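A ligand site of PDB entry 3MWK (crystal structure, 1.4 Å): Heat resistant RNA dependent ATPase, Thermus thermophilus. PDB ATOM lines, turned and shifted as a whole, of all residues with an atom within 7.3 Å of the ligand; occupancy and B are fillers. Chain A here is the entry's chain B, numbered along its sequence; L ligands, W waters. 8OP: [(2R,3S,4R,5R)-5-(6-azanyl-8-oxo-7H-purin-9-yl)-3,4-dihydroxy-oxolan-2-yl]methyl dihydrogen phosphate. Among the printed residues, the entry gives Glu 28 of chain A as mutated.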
ATOM      1  N   PHE A   3      21.420  30.274  36.372  1.00  0.00           N
ATOM      2  CA  PHE A   3      20.732  29.005  36.475  1.00  0.00           C
ATOM      3  C   PHE A   3      19.893  28.855  37.763  1.00  0.00           C
ATOM      4  O   PHE A   3      18.824  28.231  37.677  1.00  0.00           O
ATOM      5  CB  PHE A   3      21.707  27.827  36.301  1.00  0.00           C
ATOM      6  CG  PHE A   3      22.232  27.671  34.924  1.00  0.00           C
ATOM      7  CD1 PHE A   3      21.369  27.488  33.863  1.00  0.00           C
ATOM      8  CD2 PHE A   3      23.604  27.699  34.671  1.00  0.00           C
ATOM      9  CE1 PHE A   3      21.837  27.385  32.569  1.00  0.00           C
ATOM     10  CE2 PHE A   3      24.083  27.596  33.368  1.00  0.00           C
ATOM     11  CZ  PHE A   3      23.185  27.400  32.333  1.00  0.00           C
ATOM     12  N   LEU A  16      25.175  21.716  38.809  1.00  0.00           N
ATOM     13  CA  LEU A  16      25.703  22.928  38.125  1.00  0.00           C
ATOM     14  C   LEU A  16      26.737  23.734  38.946  1.00  0.00           C
ATOM     15  O   LEU A  16      27.809  24.067  38.446  1.00  0.00           O
ATOM     16  CB  LEU A  16      24.553  23.869  37.724  1.00  0.00           C
ATOM     17  CG  LEU A  16      23.662  23.390  36.584  1.00  0.00           C
ATOM     18  CD1 LEU A  16      22.349  24.181  36.573  1.00  0.00           C
ATOM     19  CD2 LEU A  16      24.384  23.508  35.227  1.00  0.00           C
ATOM     20  N   ARG A  19      30.200  22.396  39.220  1.00  0.00           N
ATOM     21  CA  ARG A  19      30.966  22.477  37.979  1.00  0.00           C
ATOM     22  C   ARG A  19      31.309  23.920  37.573  1.00  0.00           C
ATOM     23  O   ARG A  19      31.883  24.128  36.499  1.00  0.00           O
ATOM     24  CB  ARG A  19      30.200  21.794  36.846  1.00  0.00           C
ATOM     25  CG  ARG A  19      29.669  20.418  37.172  1.00  0.00           C
ATOM     26  CD  ARG A  19      29.536  19.605  35.907  1.00  0.00           C
ATOM     27  NE  ARG A  19      30.850  19.330  35.332  1.00  0.00           N
ATOM     28  CZ  ARG A  19      31.147  19.297  34.035  1.00  0.00           C
ATOM     29  NH1 ARG A  19      32.400  19.029  33.659  1.00  0.00           N
ATOM     30  NH2 ARG A  19      30.220  19.540  33.091  1.00  0.00           N
ATOM     31  N   GLY A  20      30.966  24.911  38.408  1.00  0.00           N
ATOM     32  CA  GLY A  20      31.175  26.332  38.076  1.00  0.00           C
ATOM     33  C   GLY A  20      30.302  26.806  36.935  1.00  0.00           C
ATOM     34  O   GLY A  20      30.653  27.733  36.221  1.00  0.00           O
ATOM     35  N   LEU A  21      29.187  26.129  36.731  1.00  0.00           N
ATOM     36  CA  LEU A  21      28.197  26.509  35.713  1.00  0.00           C
ATOM     37  C   LEU A  21      27.123  27.362  36.404  1.00  0.00           C
ATOM     38  O   LEU A  21      26.342  26.854  37.183  1.00  0.00           O
ATOM     39  CB  LEU A  21      27.607  25.255  35.054  1.00  0.00           C
ATOM     40  CG  LEU A  21      28.529  24.436  34.125  1.00  0.00           C
ATOM     41  CD1 LEU A  21      27.822  23.166  33.630  1.00  0.00           C
ATOM     42  CD2 LEU A  21      29.037  25.247  32.893  1.00  0.00           C
ATOM     43  N   THR A  22      27.144  28.653  36.122  1.00  0.00           N
ATOM     44  CA  THR A  22      26.346  29.652  36.834  1.00  0.00           C
ATOM     45  C   THR A  22      25.395  30.428  35.907  1.00  0.00           C
ATOM     46  O   THR A  22      24.289  30.786  36.311  1.00  0.00           O
ATOM     47  CB  THR A  22      27.245  30.730  37.546  1.00  0.00           C
ATOM     48  OG1 THR A  22      27.984  31.455  36.552  1.00  0.00           O
ATOM     49  CG2 THR A  22      28.218  30.100  38.577  1.00  0.00           C
ATOM     50  N   THR A  23      25.853  30.684  34.673  1.00  0.00           N
ATOM     51  CA  THR A  23      25.254  31.667  33.774  1.00  0.00           C
ATOM     52  C   THR A  23      24.910  31.066  32.396  1.00  0.00           C
ATOM     53  O   THR A  23      25.811  30.655  31.607  1.00  0.00           O
ATOM     54  CB  THR A  23      26.205  32.866  33.556  1.00  0.00           C
ATOM     55  OG1 THR A  23      26.585  33.416  34.841  1.00  0.00           O
ATOM     56  CG2 THR A  23      25.545  33.967  32.706  1.00  0.00           C
ATOM     57  N   PRO A  24      23.596  31.012  32.068  1.00  0.00           N
ATOM     58  CA  PRO A  24      23.232  30.537  30.750  1.00  0.00           C
ATOM     59  C   PRO A  24      23.814  31.465  29.676  1.00  0.00           C
ATOM     60  O   PRO A  24      23.847  32.694  29.843  1.00  0.00           O
ATOM     61  CB  PRO A  24      21.700  30.613  30.736  1.00  0.00           C
ATOM     62  CG  PRO A  24      21.315  31.040  32.096  1.00  0.00           C
ATOM     63  CD  PRO A  24      22.461  31.592  32.788  1.00  0.00           C
ATOM     64  N   THR A  25      24.237  30.877  28.579  1.00  0.00           N
ATOM     65  CA  THR A  25      24.551  31.658  27.401  1.00  0.00           C
ATOM     66  C   THR A  25      23.209  32.234  26.863  1.00  0.00           C
ATOM     67  O   THR A  25      22.098  31.760  27.201  1.00  0.00           O
ATOM     68  CB  THR A  25      25.210  30.797  26.313  1.00  0.00           C
ATOM     69  OG1 THR A  25      24.264  29.835  25.907  1.00  0.00           O
ATOM     70  CG2 THR A  25      26.583  30.105  26.802  1.00  0.00           C
ATOM     71  N   PRO A  26      23.291  33.259  26.015  1.00  0.00           N
ATOM     72  CA  PRO A  26      22.032  33.844  25.582  1.00  0.00           C
ATOM     73  C   PRO A  26      21.037  32.829  24.953  1.00  0.00           C
ATOM     74  O   PRO A  26      19.817  32.896  25.231  1.00  0.00           O
ATOM     75  CB  PRO A  26      22.493  34.890  24.556  1.00  0.00           C
ATOM     76  CG  PRO A  26      23.818  35.352  25.098  1.00  0.00           C
ATOM     77  CD  PRO A  26      24.465  34.067  25.620  1.00  0.00           C
ATOM     78  N   GLU A  28      20.732  29.693  25.632  1.00  0.00           N
ATOM     79  CA  GLU A  28      20.230  28.927  26.778  1.00  0.00           C
ATOM     80  C   GLU A  28      19.173  29.747  27.568  1.00  0.00           C
ATOM     81  O   GLU A  28      18.149  29.208  27.996  1.00  0.00           O
ATOM     82  CB  GLU A  28      21.371  28.536  27.688  1.00  0.00           C
ATOM     83  CG  GLU A  28      22.308  27.534  26.988  1.00  0.00           C
ATOM     84  CD  GLU A  28      23.546  27.208  27.764  1.00  0.00           C
ATOM     85  OE1 GLU A  28      23.887  27.987  28.703  1.00  0.00           O
ATOM     86  OE2 GLU A  28      24.157  26.134  27.417  1.00  0.00           O
ATOM     87  N   ARG A  46      26.125  30.246  16.237  1.00  0.00           N
ATOM     88  CA  ARG A  46      27.401  29.985  15.572  1.00  0.00           C
ATOM     89  C   ARG A  46      27.924  28.632  15.997  1.00  0.00           C
ATOM     90  O   ARG A  46      27.892  28.304  17.181  1.00  0.00           O
ATOM     91  CB  ARG A  46      28.455  31.060  15.906  1.00  0.00           C
ATOM     92  CG  ARG A  46      28.556  32.183  14.854  1.00  0.00           C
ATOM     93  CD  ARG A  46      29.423  33.361  15.351  1.00  0.00           C
ATOM     94  NE  ARG A  46      28.687  34.260  16.248  1.00  0.00           N
ATOM     95  CZ  ARG A  46      29.226  35.161  17.077  1.00  0.00           C
ATOM     96  NH1 ARG A  46      30.550  35.345  17.151  1.00  0.00           N
ATOM     97  NH2 ARG A  46      28.438  35.914  17.840  1.00  0.00           N
ATOM     98  N   THR A  47      28.417  27.846  15.022  1.00  0.00           N
ATOM     99  CA  THR A  47      28.774  26.455  15.287  1.00  0.00           C
ATOM    100  C   THR A  47      29.753  26.355  16.456  1.00  0.00           C
ATOM    101  O   THR A  47      30.626  27.221  16.655  1.00  0.00           O
ATOM    102  CB  THR A  47      29.380  25.749  14.053  1.00  0.00           C
ATOM    103  OG1 THR A  47      29.609  24.364  14.369  1.00  0.00           O
ATOM    104  CG2 THR A  47      30.680  26.434  13.646  1.00  0.00           C
ATOM    105  N   GLY A  48      29.561  25.304  17.262  1.00  0.00           N
ATOM    106  CA  GLY A  48      30.419  25.070  18.428  1.00  0.00           C
ATOM    107  C   GLY A  48      30.147  26.006  19.600  1.00  0.00           C
ATOM    108  O   GLY A  48      30.680  25.786  20.686  1.00  0.00           O
ATOM    109  N   THR A  49      29.330  27.056  19.400  1.00  0.00           N
ATOM    110  CA  THR A  49      28.955  27.973  20.496  1.00  0.00           C
ATOM    111  C   THR A  49      28.194  27.255  21.620  1.00  0.00           C
ATOM    112  O   THR A  49      27.569  26.196  21.432  1.00  0.00           O
ATOM    113  CB  THR A  49      28.080  29.177  20.002  1.00  0.00           C
ATOM    114  OG1 THR A  49      28.090  30.217  20.987  1.00  0.00           O
ATOM    115  CG2 THR A  49      26.628  28.748  19.736  1.00  0.00           C
ATOM    116  N   GLY A  50      28.266  27.825  22.810  1.00  0.00           N
ATOM    117  CA  GLY A  50      27.783  27.000  23.904  1.00  0.00           C
ATOM    118  C   GLY A  50      26.283  26.998  24.056  1.00  0.00           C
ATOM    119  O   GLY A  50      25.684  28.035  24.252  1.00  0.00           O
ATOM    120  N   LYS A  51      25.660  25.813  23.932  1.00  0.00           N
ATOM    121  CA  LYS A  51      24.204  25.677  24.057  1.00  0.00           C
ATOM    122  C   LYS A  51      23.804  24.361  24.740  1.00  0.00           C
ATOM    123  O   LYS A  51      22.628  24.014  24.747  1.00  0.00           O
ATOM    124  CB  LYS A  51      23.559  25.775  22.653  1.00  0.00           C
ATOM    125  CG  LYS A  51      24.074  24.757  21.590  1.00  0.00           C
ATOM    126  CD  LYS A  51      23.538  23.357  21.788  1.00  0.00           C
ATOM    127  CE  LYS A  51      23.887  22.436  20.624  1.00  0.00           C
ATOM    128  NZ  LYS A  51      25.400  22.207  20.497  1.00  0.00           N
ATOM    129  N   THR A  52      24.764  23.618  25.271  1.00  0.00           N
ATOM    130  CA  THR A  52      24.453  22.282  25.751  1.00  0.00           C
ATOM    131  C   THR A  52      23.390  22.243  26.838  1.00  0.00           C
ATOM    132  O   THR A  52      22.535  21.333  26.882  1.00  0.00           O
ATOM    133  CB  THR A  52      25.726  21.458  26.157  1.00  0.00           C
ATOM    134  OG1 THR A  52      26.610  21.376  25.028  1.00  0.00           O
ATOM    135  CG2 THR A  52      25.369  20.058  26.722  1.00  0.00           C
ATOM    136  N   LEU A  53      23.420  23.237  27.702  1.00  0.00           N
ATOM    137  CA  LEU A  53      22.489  23.263  28.833  1.00  0.00           C
ATOM    138  C   LEU A  53      21.042  23.563  28.380  1.00  0.00           C
ATOM    139  O   LEU A  53      20.128  23.309  29.114  1.00  0.00           O
ATOM    140  CB  LEU A  53      22.998  24.211  29.927  1.00  0.00           C
ATOM    141  CG  LEU A  53      24.415  23.785  30.399  1.00  0.00           C
ATOM    142  CD1 LEU A  53      25.093  24.808  31.280  1.00  0.00           C
ATOM    143  CD2 LEU A  53      24.430  22.406  31.033  1.00  0.00           C
ATOM    144  N   ALA A  54      20.853  24.101  27.151  1.00  0.00           N
ATOM    145  CA  ALA A  54      19.532  24.327  26.595  1.00  0.00           C
ATOM    146  C   ALA A  54      18.775  23.044  26.413  1.00  0.00           C
ATOM    147  O   ALA A  54      17.498  23.050  26.398  1.00  0.00           O
ATOM    148  CB  ALA A  54      19.611  25.082  25.256  1.00  0.00           C
ATOM    149  N   PHE A  55      19.483  21.944  26.197  1.00  0.00           N
ATOM    150  CA  PHE A  55      18.789  20.652  26.172  1.00  0.00           C
ATOM    151  C   PHE A  55      19.149  19.740  27.344  1.00  0.00           C
ATOM    152  O   PHE A  55      18.313  18.931  27.710  1.00  0.00           O
ATOM    153  CB  PHE A  55      18.971  19.895  24.857  1.00  0.00           C
ATOM    154  CG  PHE A  55      20.423  19.524  24.515  1.00  0.00           C
ATOM    155  CD1 PHE A  55      20.946  18.298  24.950  1.00  0.00           C
ATOM    156  CD2 PHE A  55      21.212  20.332  23.744  1.00  0.00           C
ATOM    157  CE1 PHE A  55      22.231  17.914  24.598  1.00  0.00           C
ATOM    158  CE2 PHE A  55      22.501  19.990  23.427  1.00  0.00           C
ATOM    159  CZ  PHE A  55      23.011  18.792  23.829  1.00  0.00           C
ATOM    160  N   LEU A  84      31.937  14.607  19.678  1.00  0.00           N
ATOM    161  CA  LEU A  84      30.785  15.338  20.227  1.00  0.00           C
ATOM    162  C   LEU A  84      29.889  14.428  21.061  1.00  0.00           C
ATOM    163  O   LEU A  84      29.438  14.854  22.139  1.00  0.00           O
ATOM    164  CB  LEU A  84      29.967  16.029  19.154  1.00  0.00           C
ATOM    165  CG  LEU A  84      30.687  17.170  18.454  1.00  0.00           C
ATOM    166  CD1 LEU A  84      29.887  17.753  17.288  1.00  0.00           C
ATOM    167  CD2 LEU A  84      31.082  18.265  19.410  1.00  0.00           C
ATOM    168  N   GLN A  87      31.664  14.188  24.438  1.00  0.00           N
ATOM    169  CA  GLN A  87      31.622  15.495  25.096  1.00  0.00           C
ATOM    170  C   GLN A  87      30.192  15.808  25.624  1.00  0.00           C
ATOM    171  O   GLN A  87      30.008  16.154  26.804  1.00  0.00           O
ATOM    172  CB  GLN A  87      32.087  16.583  24.135  1.00  0.00           C
ATOM    173  CG  GLN A  87      32.101  18.015  24.597  1.00  0.00           C
ATOM    174  CD  GLN A  87      33.191  18.394  25.577  1.00  0.00           C
ATOM    175  OE1 GLN A  87      33.613  17.612  26.445  1.00  0.00           O
ATOM    176  NE2 GLN A  87      33.655  19.626  25.446  1.00  0.00           N
ATOM    177  N   VAL A  88      29.194  15.700  24.750  1.00  0.00           N
ATOM    178  CA  VAL A  88      27.802  15.864  25.204  1.00  0.00           C
ATOM    179  C   VAL A  88      27.370  14.864  26.302  1.00  0.00           C
ATOM    180  O   VAL A  88      26.754  15.280  27.281  1.00  0.00           O
ATOM    181  CB  VAL A  88      26.858  15.763  24.040  1.00  0.00           C
ATOM    182  CG1 VAL A  88      25.345  15.802  24.513  1.00  0.00           C
ATOM    183  CG2 VAL A  88      27.156  16.927  23.029  1.00  0.00           C
ATOM    184  N   GLU A  91      28.777  15.924  29.555  1.00  0.00           N
ATOM    185  CA  GLU A  91      28.110  17.117  30.098  1.00  0.00           C
ATOM    186  C   GLU A  91      26.739  16.744  30.655  1.00  0.00           C
ATOM    187  O   GLU A  91      26.338  17.256  31.703  1.00  0.00           O
ATOM    188  CB  GLU A  91      28.004  18.239  29.066  1.00  0.00           C
ATOM    189  CG  GLU A  91      29.358  18.923  28.877  1.00  0.00           C
ATOM    190  CD  GLU A  91      29.351  20.012  27.835  1.00  0.00           C
ATOM    191  OE1 GLU A  91      28.399  20.845  27.780  1.00  0.00           O
ATOM    192  OE2 GLU A  91      30.356  20.070  27.084  1.00  0.00           O
HETATM  193  P   8OP L   1      33.159  27.434  23.237  1.00  0.00           P
HETATM  194  O1P 8OP L   1      32.061  28.342  22.555  1.00  0.00           O
HETATM  195  O2P 8OP L   1      34.196  28.263  24.051  1.00  0.00           O
HETATM  196  O3P 8OP L   1      33.737  26.328  22.289  1.00  0.00           O
HETATM  197  O50 8OP L   1      32.332  26.634  24.394  1.00  0.00           O
HETATM  198  C50 8OP L   1      31.485  25.561  24.040  1.00  0.00           C
HETATM  199  C40 8OP L   1      31.264  24.798  25.333  1.00  0.00           C
HETATM  200  O40 8OP L   1      30.733  25.606  26.401  1.00  0.00           O
HETATM  201  C30 8OP L   1      30.189  23.750  25.140  1.00  0.00           C
HETATM  202  O30 8OP L   1      30.679  22.685  24.314  1.00  0.00           O
HETATM  203  C20 8OP L   1      30.029  23.403  26.619  1.00  0.00           C
HETATM  204  O20 8OP L   1      31.086  22.531  26.924  1.00  0.00           O
HETATM  205  C10 8OP L   1      30.239  24.695  27.383  1.00  0.00           C
HETATM  206  N9  8OP L   1      28.981  25.238  27.977  1.00  0.00           N
HETATM  207  C8  8OP L   1      27.664  25.184  27.412  1.00  0.00           C
HETATM  208  O8  8OP L   1      27.317  24.438  26.467  1.00  0.00           O
HETATM  209  N7  8OP L   1      26.766  26.048  28.133  1.00  0.00           N
HETATM  210  C5  8OP L   1      27.593  26.693  29.126  1.00  0.00           C
HETATM  211  C6  8OP L   1      27.341  27.651  30.095  1.00  0.00           C
HETATM  212  N6  8OP L   1      26.090  28.264  30.300  1.00  0.00           N
HETATM  213  N1  8OP L   1      28.354  28.058  30.864  1.00  0.00           N
HETATM  214  C2  8OP L   1      29.608  27.573  30.713  1.00  0.00           C
HETATM  215  N3  8OP L   1      29.926  26.638  29.812  1.00  0.00           N
HETATM  216  C4  8OP L   1      28.901  26.192  29.031  1.00  0.00           C
HETATM  217  O   HOH W   1      29.528  23.390  21.802  1.00  0.00           O
HETATM  218  O   HOH W   2      28.243  29.391  33.480  1.00  0.00           O
HETATM  219  O   HOH W   3      28.864  20.143  24.930  1.00  0.00           O
HETATM  220  O   HOH W   4      29.741  28.456  26.570  1.00  0.00           O
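Water W1 lies within hydrogen-bond range of an oxygen (O30) of the ligand (2.9 Å), the backbone carbonyl oxygen of Gly 48 (2.9 Å) and the backbone carbonyl oxygen of Thr 49 (3.4 Å). Water W2 lies within hydrogen-bond range of a nitrogen (N1) of the ligand, the backbone NH (N) of Thr 22 and the backbone NH (N) of Thr 23. Water W3 lies within hydrogen-bond range of the side-chain hydroxyl of Thr 52, the side-chain carboxylate of Glu 91 and an oxygen (O30) of the ligand.
The side-chain carboxylate (OE1) of Glu 91 lies close to the side-chain hydroxyl (OG1) of Thr 52, 3.3 Å away. The side-chain carboxylate (OE2) of Glu 28 sits at hydrogen-bond distance from the backbone NH (N) of Thr 52 (3.4 Å). The backbone NH (N) of Thr 25 sits at hydrogen-bond distance from the side-chain carboxylate (OE1) of Glu 28, at 2.9 Å. N of Leu 53 is in hydrogen-bond range of OE2 of Glu 28 (3.0 Å). OG1 of Thr 23 sits at hydrogen-bond distance from OG1 of Thr 22, 3.0 Å away. The backbone NH (N) of Leu 21 sits at hydrogen-bond distance from the backbone carbonyl oxygen (O) of Leu 16. The side-chain hydroxyl (OG1) of Thr 25 sits at hydrogen-bond distance from the backbone carbonyl oxygen (O) of Gly 50 (2.8 Å). The backbone carbonyl oxygen of Thr 22 is in hydrogen-bond range of the backbone NH of Phe 3, at 2.9 Å.
O1P of the ligand lies close to O of Gly 48 (3.5 Å). Residues that only touch the ligand: Phe 3 (3.6 Å), Leu 21 (3.2 Å), Pro 24 (3.7 Å), Thr 25 (3.6 Å), Thr 49 (3.7 Å), Gly 50 (3.7 Å) and Leu 53 (3.7 Å). Hydrophobic or aromatic side chains that line the ligand: Phe 3, Leu 21 and Leu 53.
The side-chain carboxylate of Glu 91 is in hydrogen-bond range of an oxygen (O20) of the ligand. OE2 of Glu 28 lies within hydrogen-bond range of N7 of the ligand (2.7 Å). The backbone carbonyl oxygen (O) of Thr 23 lies within hydrogen-bond range of a nitrogen (N6) of the ligand, at 2.7 Å. The backbone NH (N) of Thr 52 lies within hydrogen-bond range of an oxygen (O8) of the ligand, at 2.9 Å. The side-chain hydroxyl (OG1) of Thr 52 sits close to an oxygen (O8) of the ligand, at 3.5 Å. The backbone NH (N) of Lys 51 sits at hydrogen-bond distance from an oxygen (O8) of the ligand (3.3 Å).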
